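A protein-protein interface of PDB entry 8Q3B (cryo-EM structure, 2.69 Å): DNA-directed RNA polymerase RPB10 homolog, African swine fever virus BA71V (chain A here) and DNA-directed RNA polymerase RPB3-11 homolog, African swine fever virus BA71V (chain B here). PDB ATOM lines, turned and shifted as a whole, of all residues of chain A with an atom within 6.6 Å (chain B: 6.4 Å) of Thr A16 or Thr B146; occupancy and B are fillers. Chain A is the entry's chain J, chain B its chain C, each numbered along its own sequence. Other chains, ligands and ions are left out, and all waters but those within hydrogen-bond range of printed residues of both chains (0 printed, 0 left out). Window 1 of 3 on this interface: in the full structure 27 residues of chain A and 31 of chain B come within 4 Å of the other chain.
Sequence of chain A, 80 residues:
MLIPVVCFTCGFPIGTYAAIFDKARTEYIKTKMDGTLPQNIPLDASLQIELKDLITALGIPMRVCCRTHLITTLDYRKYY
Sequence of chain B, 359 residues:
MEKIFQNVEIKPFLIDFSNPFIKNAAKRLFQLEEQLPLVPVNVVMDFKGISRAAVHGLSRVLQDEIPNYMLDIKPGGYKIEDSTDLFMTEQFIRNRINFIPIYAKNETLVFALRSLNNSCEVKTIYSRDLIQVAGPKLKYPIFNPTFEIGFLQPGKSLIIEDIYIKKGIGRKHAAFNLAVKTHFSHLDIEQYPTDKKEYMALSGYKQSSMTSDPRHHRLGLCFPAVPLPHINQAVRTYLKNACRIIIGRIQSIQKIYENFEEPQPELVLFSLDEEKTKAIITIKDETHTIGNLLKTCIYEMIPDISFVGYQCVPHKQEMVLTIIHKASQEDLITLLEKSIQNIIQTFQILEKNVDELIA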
ATOM      1  N   PRO A   4      17.877   2.967  22.139  1.00  0.00           N
ATOM      2  CA  PRO A   4      16.529   2.485  21.821  1.00  0.00           C
ATOM      3  C   PRO A   4      16.552   1.414  20.742  1.00  0.00           C
ATOM      4  O   PRO A   4      17.419   1.397  19.867  1.00  0.00           O
ATOM      5  CB  PRO A   4      15.798   3.748  21.346  1.00  0.00           C
ATOM      6  CG  PRO A   4      16.867   4.726  21.013  1.00  0.00           C
ATOM      7  CD  PRO A   4      18.004   4.418  21.924  1.00  0.00           C
ATOM      8  N   VAL A   5      15.579   0.504  20.824  1.00  0.00           N
ATOM      9  CA  VAL A   5      15.505  -0.593  19.864  1.00  0.00           C
ATOM     10  C   VAL A   5      15.386  -0.047  18.448  1.00  0.00           C
ATOM     11  O   VAL A   5      16.037  -0.540  17.519  1.00  0.00           O
ATOM     12  CB  VAL A   5      14.330  -1.524  20.214  1.00  0.00           C
ATOM     13  CG1 VAL A   5      14.082  -2.515  19.090  1.00  0.00           C
ATOM     14  CG2 VAL A   5      14.603  -2.252  21.517  1.00  0.00           C
ATOM     15  N   VAL A   6      14.552   0.972  18.259  1.00  0.00           N
ATOM     16  CA  VAL A   6      14.374   1.619  16.968  1.00  0.00           C
ATOM     17  C   VAL A   6      14.618   3.109  17.136  1.00  0.00           C
ATOM     18  O   VAL A   6      14.423   3.672  18.218  1.00  0.00           O
ATOM     19  CB  VAL A   6      12.967   1.368  16.382  1.00  0.00           C
ATOM     20  CG1 VAL A   6      12.794  -0.094  16.024  1.00  0.00           C
ATOM     21  CG2 VAL A   6      11.896   1.810  17.365  1.00  0.00           C
ATOM     22  N   PRO A  13      15.647   0.375  12.723  1.00  0.00           N
ATOM     23  CA  PRO A  13      16.120  -0.453  13.841  1.00  0.00           C
ATOM     24  C   PRO A  13      17.608  -0.298  14.113  1.00  0.00           C
ATOM     25  O   PRO A  13      18.403  -1.180  13.777  1.00  0.00           O
ATOM     26  CB  PRO A  13      15.779  -1.874  13.384  1.00  0.00           C
ATOM     27  CG  PRO A  13      15.825  -1.804  11.906  1.00  0.00           C
ATOM     28  CD  PRO A  13      15.306  -0.442  11.546  1.00  0.00           C
ATOM     29  N   ILE A  14      17.995   0.824  14.724  1.00  0.00           N
ATOM     30  CA  ILE A  14      19.390   1.006  15.106  1.00  0.00           C
ATOM     31  C   ILE A  14      19.778   0.019  16.198  1.00  0.00           C
ATOM     32  O   ILE A  14      20.930  -0.431  16.258  1.00  0.00           O
ATOM     33  CB  ILE A  14      19.643   2.460  15.547  1.00  0.00           C
ATOM     34  CG1 ILE A  14      18.718   2.846  16.704  1.00  0.00           C
ATOM     35  CG2 ILE A  14      19.455   3.405  14.372  1.00  0.00           C
ATOM     36  CD1 ILE A  14      19.005   4.209  17.292  1.00  0.00           C
ATOM     37  N   GLY A  15      18.832  -0.350  17.062  1.00  0.00           N
ATOM     38  CA  GLY A  15      19.158  -1.212  18.184  1.00  0.00           C
ATOM     39  C   GLY A  15      19.831  -2.504  17.772  1.00  0.00           C
ATOM     40  O   GLY A  15      20.663  -3.037  18.511  1.00  0.00           O
ATOM     41  N   THR A  16      19.509  -3.009  16.579  1.00  0.00           N
ATOM     42  CA  THR A  16      20.100  -4.261  16.121  1.00  0.00           C
ATOM     43  C   THR A  16      21.618  -4.220  16.191  1.00  0.00           C
ATOM     44  O   THR A  16      22.257  -5.248  16.439  1.00  0.00           O
ATOM     45  CB  THR A  16      19.661  -4.558  14.686  1.00  0.00           C
ATOM     46  OG1 THR A  16      18.320  -4.097  14.485  1.00  0.00           O
ATOM     47  CG2 THR A  16      19.733  -6.048  14.402  1.00  0.00           C
ATOM     48  N   TYR A  17      22.211  -3.047  15.975  1.00  0.00           N
ATOM     49  CA  TYR A  17      23.657  -2.889  16.034  1.00  0.00           C
ATOM     50  C   TYR A  17      24.131  -2.209  17.309  1.00  0.00           C
ATOM     51  O   TYR A  17      25.338  -2.212  17.578  1.00  0.00           O
ATOM     52  CB  TYR A  17      24.142  -2.087  14.823  1.00  0.00           C
ATOM     53  CG  TYR A  17      23.416  -2.425  13.542  1.00  0.00           C
ATOM     54  CD1 TYR A  17      23.828  -3.486  12.749  1.00  0.00           C
ATOM     55  CD2 TYR A  17      22.319  -1.684  13.126  1.00  0.00           C
ATOM     56  CE1 TYR A  17      23.169  -3.801  11.579  1.00  0.00           C
ATOM     57  CE2 TYR A  17      21.653  -1.992  11.957  1.00  0.00           C
ATOM     58  CZ  TYR A  17      22.082  -3.051  11.187  1.00  0.00           C
ATOM     59  OH  TYR A  17      21.425  -3.363  10.021  1.00  0.00           O
ATOM     60  N   ALA A  18      23.214  -1.653  18.106  1.00  0.00           N
ATOM     61  CA  ALA A  18      23.587  -0.853  19.265  1.00  0.00           C
ATOM     62  C   ALA A  18      24.724  -1.490  20.053  1.00  0.00           C
ATOM     63  O   ALA A  18      25.814  -0.917  20.171  1.00  0.00           O
ATOM     64  CB  ALA A  18      22.365  -0.646  20.164  1.00  0.00           C
ATOM     65  N   ALA A  19      24.495  -2.700  20.565  1.00  0.00           N
ATOM     66  CA  ALA A  19      25.501  -3.347  21.398  1.00  0.00           C
ATOM     67  C   ALA A  19      26.851  -3.367  20.697  1.00  0.00           C
ATOM     68  O   ALA A  19      27.853  -2.880  21.237  1.00  0.00           O
ATOM     69  CB  ALA A  19      25.057  -4.767  21.750  1.00  0.00           C
ATOM     70  N   ILE A  20      26.881  -3.864  19.458  1.00  0.00           N
ATOM     71  CA  ILE A  20      28.146  -3.943  18.733  1.00  0.00           C
ATOM     72  C   ILE A  20      28.794  -2.569  18.694  1.00  0.00           C
ATOM     73  O   ILE A  20      29.971  -2.402  19.042  1.00  0.00           O
ATOM     74  CB  ILE A  20      27.922  -4.503  17.317  1.00  0.00           C
ATOM     75  CG1 ILE A  20      27.461  -5.960  17.393  1.00  0.00           C
ATOM     76  CG2 ILE A  20      29.197  -4.387  16.486  1.00  0.00           C
ATOM     77  CD1 ILE A  20      27.048  -6.551  16.061  1.00  0.00           C
ATOM     78  N   PHE B  30      28.783 -11.676  19.848  1.00  0.00           N
ATOM     79  CA  PHE B  30      27.793 -12.609  19.323  1.00  0.00           C
ATOM     80  C   PHE B  30      28.404 -13.723  18.484  1.00  0.00           C
ATOM     81  O   PHE B  30      27.657 -14.481  17.853  1.00  0.00           O
ATOM     82  CB  PHE B  30      26.752 -11.857  18.485  1.00  0.00           C
ATOM     83  CG  PHE B  30      26.083 -10.732  19.218  1.00  0.00           C
ATOM     84  CD1 PHE B  30      25.264 -10.985  20.304  1.00  0.00           C
ATOM     85  CD2 PHE B  30      26.277  -9.421  18.823  1.00  0.00           C
ATOM     86  CE1 PHE B  30      24.650  -9.951  20.979  1.00  0.00           C
ATOM     87  CE2 PHE B  30      25.665  -8.385  19.496  1.00  0.00           C
ATOM     88  CZ  PHE B  30      24.852  -8.651  20.575  1.00  0.00           C
ATOM     89  N   LEU B  32      29.640 -13.463  15.735  1.00  0.00           N
ATOM     90  CA  LEU B  32      29.016 -13.169  14.452  1.00  0.00           C
ATOM     91  C   LEU B  32      30.099 -12.759  13.460  1.00  0.00           C
ATOM     92  O   LEU B  32      30.726 -11.707  13.613  1.00  0.00           O
ATOM     93  CB  LEU B  32      27.969 -12.068  14.607  1.00  0.00           C
ATOM     94  CG  LEU B  32      27.133 -11.746  13.368  1.00  0.00           C
ATOM     95  CD1 LEU B  32      26.006 -12.753  13.213  1.00  0.00           C
ATOM     96  CD2 LEU B  32      26.584 -10.333  13.453  1.00  0.00           C
ATOM     97  N   LEU B  36      23.605 -10.686   9.473  1.00  0.00           N
ATOM     98  CA  LEU B  36      22.553 -11.143  10.361  1.00  0.00           C
ATOM     99  C   LEU B  36      21.424 -11.785   9.556  1.00  0.00           C
ATOM    100  O   LEU B  36      21.247 -11.489   8.372  1.00  0.00           O
ATOM    101  CB  LEU B  36      22.016  -9.979  11.187  1.00  0.00           C
ATOM    102  CG  LEU B  36      22.946  -9.474  12.292  1.00  0.00           C
ATOM    103  CD1 LEU B  36      22.520  -8.095  12.761  1.00  0.00           C
ATOM    104  CD2 LEU B  36      22.973 -10.450  13.456  1.00  0.00           C
ATOM    105  N   LEU B  38      18.257 -11.321   9.391  1.00  0.00           N
ATOM    106  CA  LEU B  38      17.333 -10.337   8.845  1.00  0.00           C
ATOM    107  C   LEU B  38      18.059  -9.010   8.694  1.00  0.00           C
ATOM    108  O   LEU B  38      18.699  -8.539   9.640  1.00  0.00           O
ATOM    109  CB  LEU B  38      16.108 -10.173   9.747  1.00  0.00           C
ATOM    110  CG  LEU B  38      15.049 -11.272   9.640  1.00  0.00           C
ATOM    111  CD1 LEU B  38      15.453 -12.491  10.445  1.00  0.00           C
ATOM    112  CD2 LEU B  38      13.697 -10.757  10.097  1.00  0.00           C
ATOM    113  N   PRO B 101      11.776  -5.364  15.145  1.00  0.00           N
ATOM    114  CA  PRO B 101      11.241  -5.756  13.836  1.00  0.00           C
ATOM    115  C   PRO B 101      11.226  -7.269  13.689  1.00  0.00           C
ATOM    116  O   PRO B 101      12.187  -7.955  14.041  1.00  0.00           O
ATOM    117  CB  PRO B 101      12.201  -5.099  12.838  1.00  0.00           C
ATOM    118  CG  PRO B 101      12.955  -4.085  13.611  1.00  0.00           C
ATOM    119  CD  PRO B 101      13.009  -4.572  15.016  1.00  0.00           C
ATOM    120  N   TYR B 126      19.688 -10.426  25.856  1.00  0.00           N
ATOM    121  CA  TYR B 126      19.639 -10.224  24.417  1.00  0.00           C
ATOM    122  C   TYR B 126      18.442 -10.971  23.838  1.00  0.00           C
ATOM    123  O   TYR B 126      17.814 -11.794  24.508  1.00  0.00           O
ATOM    124  CB  TYR B 126      20.928 -10.718  23.754  1.00  0.00           C
ATOM    125  CG  TYR B 126      22.145  -9.882  24.071  1.00  0.00           C
ATOM    126  CD1 TYR B 126      22.254  -8.577  23.616  1.00  0.00           C
ATOM    127  CD2 TYR B 126      23.182 -10.396  24.836  1.00  0.00           C
ATOM    128  CE1 TYR B 126      23.365  -7.811  23.906  1.00  0.00           C
ATOM    129  CE2 TYR B 126      24.294  -9.637  25.133  1.00  0.00           C
ATOM    130  CZ  TYR B 126      24.381  -8.345  24.667  1.00  0.00           C
ATOM    131  OH  TYR B 126      25.488  -7.584  24.960  1.00  0.00           O
ATOM    132  N   SER B 127      18.130 -10.673  22.574  1.00  0.00           N
ATOM    133  CA  SER B 127      16.987 -11.319  21.934  1.00  0.00           C
ATOM    134  C   SER B 127      17.208 -12.813  21.748  1.00  0.00           C
ATOM    135  O   SER B 127      16.238 -13.578  21.700  1.00  0.00           O
ATOM    136  CB  SER B 127      16.690 -10.663  20.588  1.00  0.00           C
ATOM    137  OG  SER B 127      16.094  -9.394  20.770  1.00  0.00           O
ATOM    138  N   ARG B 128      18.462 -13.254  21.633  1.00  0.00           N
ATOM    139  CA  ARG B 128      18.714 -14.683  21.483  1.00  0.00           C
ATOM    140  C   ARG B 128      18.224 -15.472  22.689  1.00  0.00           C
ATOM    141  O   ARG B 128      18.028 -16.687  22.584  1.00  0.00           O
ATOM    142  CB  ARG B 128      20.206 -14.941  21.262  1.00  0.00           C
ATOM    143  CG  ARG B 128      21.100 -14.480  22.396  1.00  0.00           C
ATOM    144  CD  ARG B 128      22.556 -14.787  22.099  1.00  0.00           C
ATOM    145  NE  ARG B 128      23.450 -14.245  23.116  1.00  0.00           N
ATOM    146  CZ  ARG B 128      24.770 -14.203  23.007  1.00  0.00           C
ATOM    147  NH1 ARG B 128      25.391 -14.666  21.934  1.00  0.00           N
ATOM    148  NH2 ARG B 128      25.486 -13.684  23.999  1.00  0.00           N
ATOM    149  N   PHE B 143      13.369 -12.727  14.068  1.00  0.00           N
ATOM    150  CA  PHE B 143      13.981 -11.480  14.502  1.00  0.00           C
ATOM    151  C   PHE B 143      15.470 -11.700  14.713  1.00  0.00           C
ATOM    152  O   PHE B 143      15.930 -12.825  14.926  1.00  0.00           O
ATOM    153  CB  PHE B 143      13.342 -10.937  15.790  1.00  0.00           C
ATOM    154  CG  PHE B 143      13.180 -11.964  16.875  1.00  0.00           C
ATOM    155  CD1 PHE B 143      14.285 -12.480  17.530  1.00  0.00           C
ATOM    156  CD2 PHE B 143      11.923 -12.397  17.253  1.00  0.00           C
ATOM    157  CE1 PHE B 143      14.136 -13.419  18.529  1.00  0.00           C
ATOM    158  CE2 PHE B 143      11.770 -13.335  18.252  1.00  0.00           C
ATOM    159  CZ  PHE B 143      12.878 -13.845  18.891  1.00  0.00           C
ATOM    160  N   ASN B 144      16.223 -10.606  14.650  1.00  0.00           N
ATOM    161  CA  ASN B 144      17.659 -10.683  14.842  1.00  0.00           C
ATOM    162  C   ASN B 144      17.982 -10.980  16.307  1.00  0.00           C
ATOM    163  O   ASN B 144      17.253 -10.558  17.209  1.00  0.00           O
ATOM    164  CB  ASN B 144      18.322  -9.377  14.422  1.00  0.00           C
ATOM    165  CG  ASN B 144      18.435  -9.241  12.920  1.00  0.00           C
ATOM    166  OD1 ASN B 144      18.865 -10.165  12.234  1.00  0.00           O
ATOM    167  ND2 ASN B 144      18.039  -8.087  12.399  1.00  0.00           N
ATOM    168  N   PRO B 145      19.068 -11.704  16.573  1.00  0.00           N
ATOM    169  CA  PRO B 145      19.429 -12.044  17.956  1.00  0.00           C
ATOM    170  C   PRO B 145      20.317 -11.031  18.666  1.00  0.00           C
ATOM    171  O   PRO B 145      20.867 -11.365  19.719  1.00  0.00           O
ATOM    172  CB  PRO B 145      20.183 -13.367  17.772  1.00  0.00           C
ATOM    173  CG  PRO B 145      20.851 -13.225  16.448  1.00  0.00           C
ATOM    174  CD  PRO B 145      19.991 -12.320  15.603  1.00  0.00           C
ATOM    175  N   THR B 146      20.471  -9.817  18.137  1.00  0.00           N
ATOM    176  CA  THR B 146      21.436  -8.863  18.665  1.00  0.00           C
ATOM    177  C   THR B 146      20.811  -7.743  19.487  1.00  0.00           C
ATOM    178  O   THR B 146      21.550  -6.959  20.090  1.00  0.00           O
ATOM    179  CB  THR B 146      22.244  -8.243  17.519  1.00  0.00           C
ATOM    180  OG1 THR B 146      21.356  -7.589  16.604  1.00  0.00           O
ATOM    181  CG2 THR B 146      23.029  -9.312  16.780  1.00  0.00           C
ATOM    182  N   PHE B 147      19.486  -7.638  19.530  1.00  0.00           N
ATOM    183  CA  PHE B 147      18.858  -6.579  20.305  1.00  0.00           C
ATOM    184  C   PHE B 147      19.113  -6.785  21.792  1.00  0.00           C
ATOM    185  O   PHE B 147      19.098  -7.913  22.291  1.00  0.00           O
ATOM    186  CB  PHE B 147      17.354  -6.534  20.046  1.00  0.00           C
ATOM    187  CG  PHE B 147      16.989  -6.156  18.644  1.00  0.00           C
ATOM    188  CD1 PHE B 147      16.852  -4.829  18.285  1.00  0.00           C
ATOM    189  CD2 PHE B 147      16.766  -7.130  17.688  1.00  0.00           C
ATOM    190  CE1 PHE B 147      16.509  -4.480  16.998  1.00  0.00           C
ATOM    191  CE2 PHE B 147      16.423  -6.785  16.400  1.00  0.00           C
ATOM    192  CZ  PHE B 147      16.296  -5.459  16.055  1.00  0.00           C
ATOM    193  N   GLU B 148      19.344  -5.683  22.502  1.00  0.00           N
ATOM    194  CA  GLU B 148      19.518  -5.711  23.951  1.00  0.00           C
ATOM    195  C   GLU B 148      18.139  -5.615  24.591  1.00  0.00           C
ATOM    196  O   GLU B 148      17.581  -4.524  24.728  1.00  0.00           O
ATOM    197  CB  GLU B 148      20.420  -4.573  24.412  1.00  0.00           C
ATOM    198  CG  GLU B 148      21.870  -4.713  23.988  1.00  0.00           C
ATOM    199  CD  GLU B 148      22.648  -3.420  24.138  1.00  0.00           C
ATOM    200  OE1 GLU B 148      22.056  -2.339  23.941  1.00  0.00           O
ATOM    201  OE2 GLU B 148      23.854  -3.486  24.455  1.00  0.00           O
ATOM    202  N   ILE B 149      17.583  -6.761  24.987  1.00  0.00           N
ATOM    203  CA  ILE B 149      16.287  -6.750  25.656  1.00  0.00           C
ATOM    204  C   ILE B 149      16.374  -5.961  26.953  1.00  0.00           C
ATOM    205  O   ILE B 149      15.435  -5.248  27.327  1.00  0.00           O
ATOM    206  CB  ILE B 149      15.795  -8.190  25.902  1.00  0.00           C
ATOM    207  CG1 ILE B 149      15.634  -8.940  24.577  1.00  0.00           C
ATOM    208  CG2 ILE B 149      14.483  -8.176  26.672  1.00  0.00           C
ATOM    209  CD1 ILE B 149      14.532  -8.403  23.684  1.00  0.00           C
ATOM    210  N   PRO B 224      12.472  -2.635   7.449  1.00  0.00           N
ATOM    211  CA  PRO B 224      13.430  -2.772   8.553  1.00  0.00           C
ATOM    212  C   PRO B 224      14.029  -4.160   8.672  1.00  0.00           C
ATOM    213  O   PRO B 224      15.163  -4.289   9.148  1.00  0.00           O
ATOM    214  CB  PRO B 224      12.589  -2.420   9.793  1.00  0.00           C
ATOM    215  CG  PRO B 224      11.207  -2.052   9.278  1.00  0.00           C
ATOM    216  CD  PRO B 224      11.090  -2.692   7.941  1.00  0.00           C
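The backbone carbonyl oxygen (O) of Leu B38 lies within hydrogen-bond range of the side-chain amide nitrogen (ND2) of Asn B144. O of Phe B147 lies within hydrogen-bond range of N of Ser B127, at 2.9 Å. N of Gly A15 is in hydrogen-bond range of O of Val A5, 2.8 Å away. The side-chain hydroxyl of Thr A16 is in hydrogen-bond range of the backbone carbonyl oxygen of Pro A13.
Hydrophobic or aromatic side chains of chain B within 4 Å of the printed part of chain A: Phe B30, Leu B36, Pro B101, Phe B147 and Pro B224. Among the printed residues, no Asp or Glu carboxylate lies within 4 Å of a Lys or Arg side-chain nitrogen of the other chain.
Tyr A17 touches none of the printed residues of chain B. Of the printed residues of chain A, Leu B36 touches Thr A16. Printed residues of chain A within 4 Å of Pro B101: Pro A13 (3.6 Å). Ser B127 touches none of the printed residues of chain A. Thr B146 touches one residue of chain A. The nearest residue of chain A that does not touch Thr B146 is Gly A15 (4.3 Å).
Val A5 touches Phe B147 (CG1 to CD1, 3.7 Å). Pro A13 touches Pro B101 (CB to CG, 3.6 Å). Pro B224 touches Pro A13 (O to CG, 3.8 Å). C of Gly A15 touches CD1 of Phe B147, at 3.8 Å. Thr A16 touches Leu B36 (CG2 to CD1, 3.8 Å). Asn B144 touches Thr A16 (ND2 to CG2, 3.3 Å). CZ of Phe B147 touches OG1 of Thr A16 (2.9 Å). CB of Ala A19 touches OE2 of Glu B148, 3.2 Å away. Ile A20 touches Phe B30.
The side-chain hydroxyl (OG1) of Thr B146 is in hydrogen-bond range of the backbone carbonyl oxygen (O) of Thr A16 (2.5 Å).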
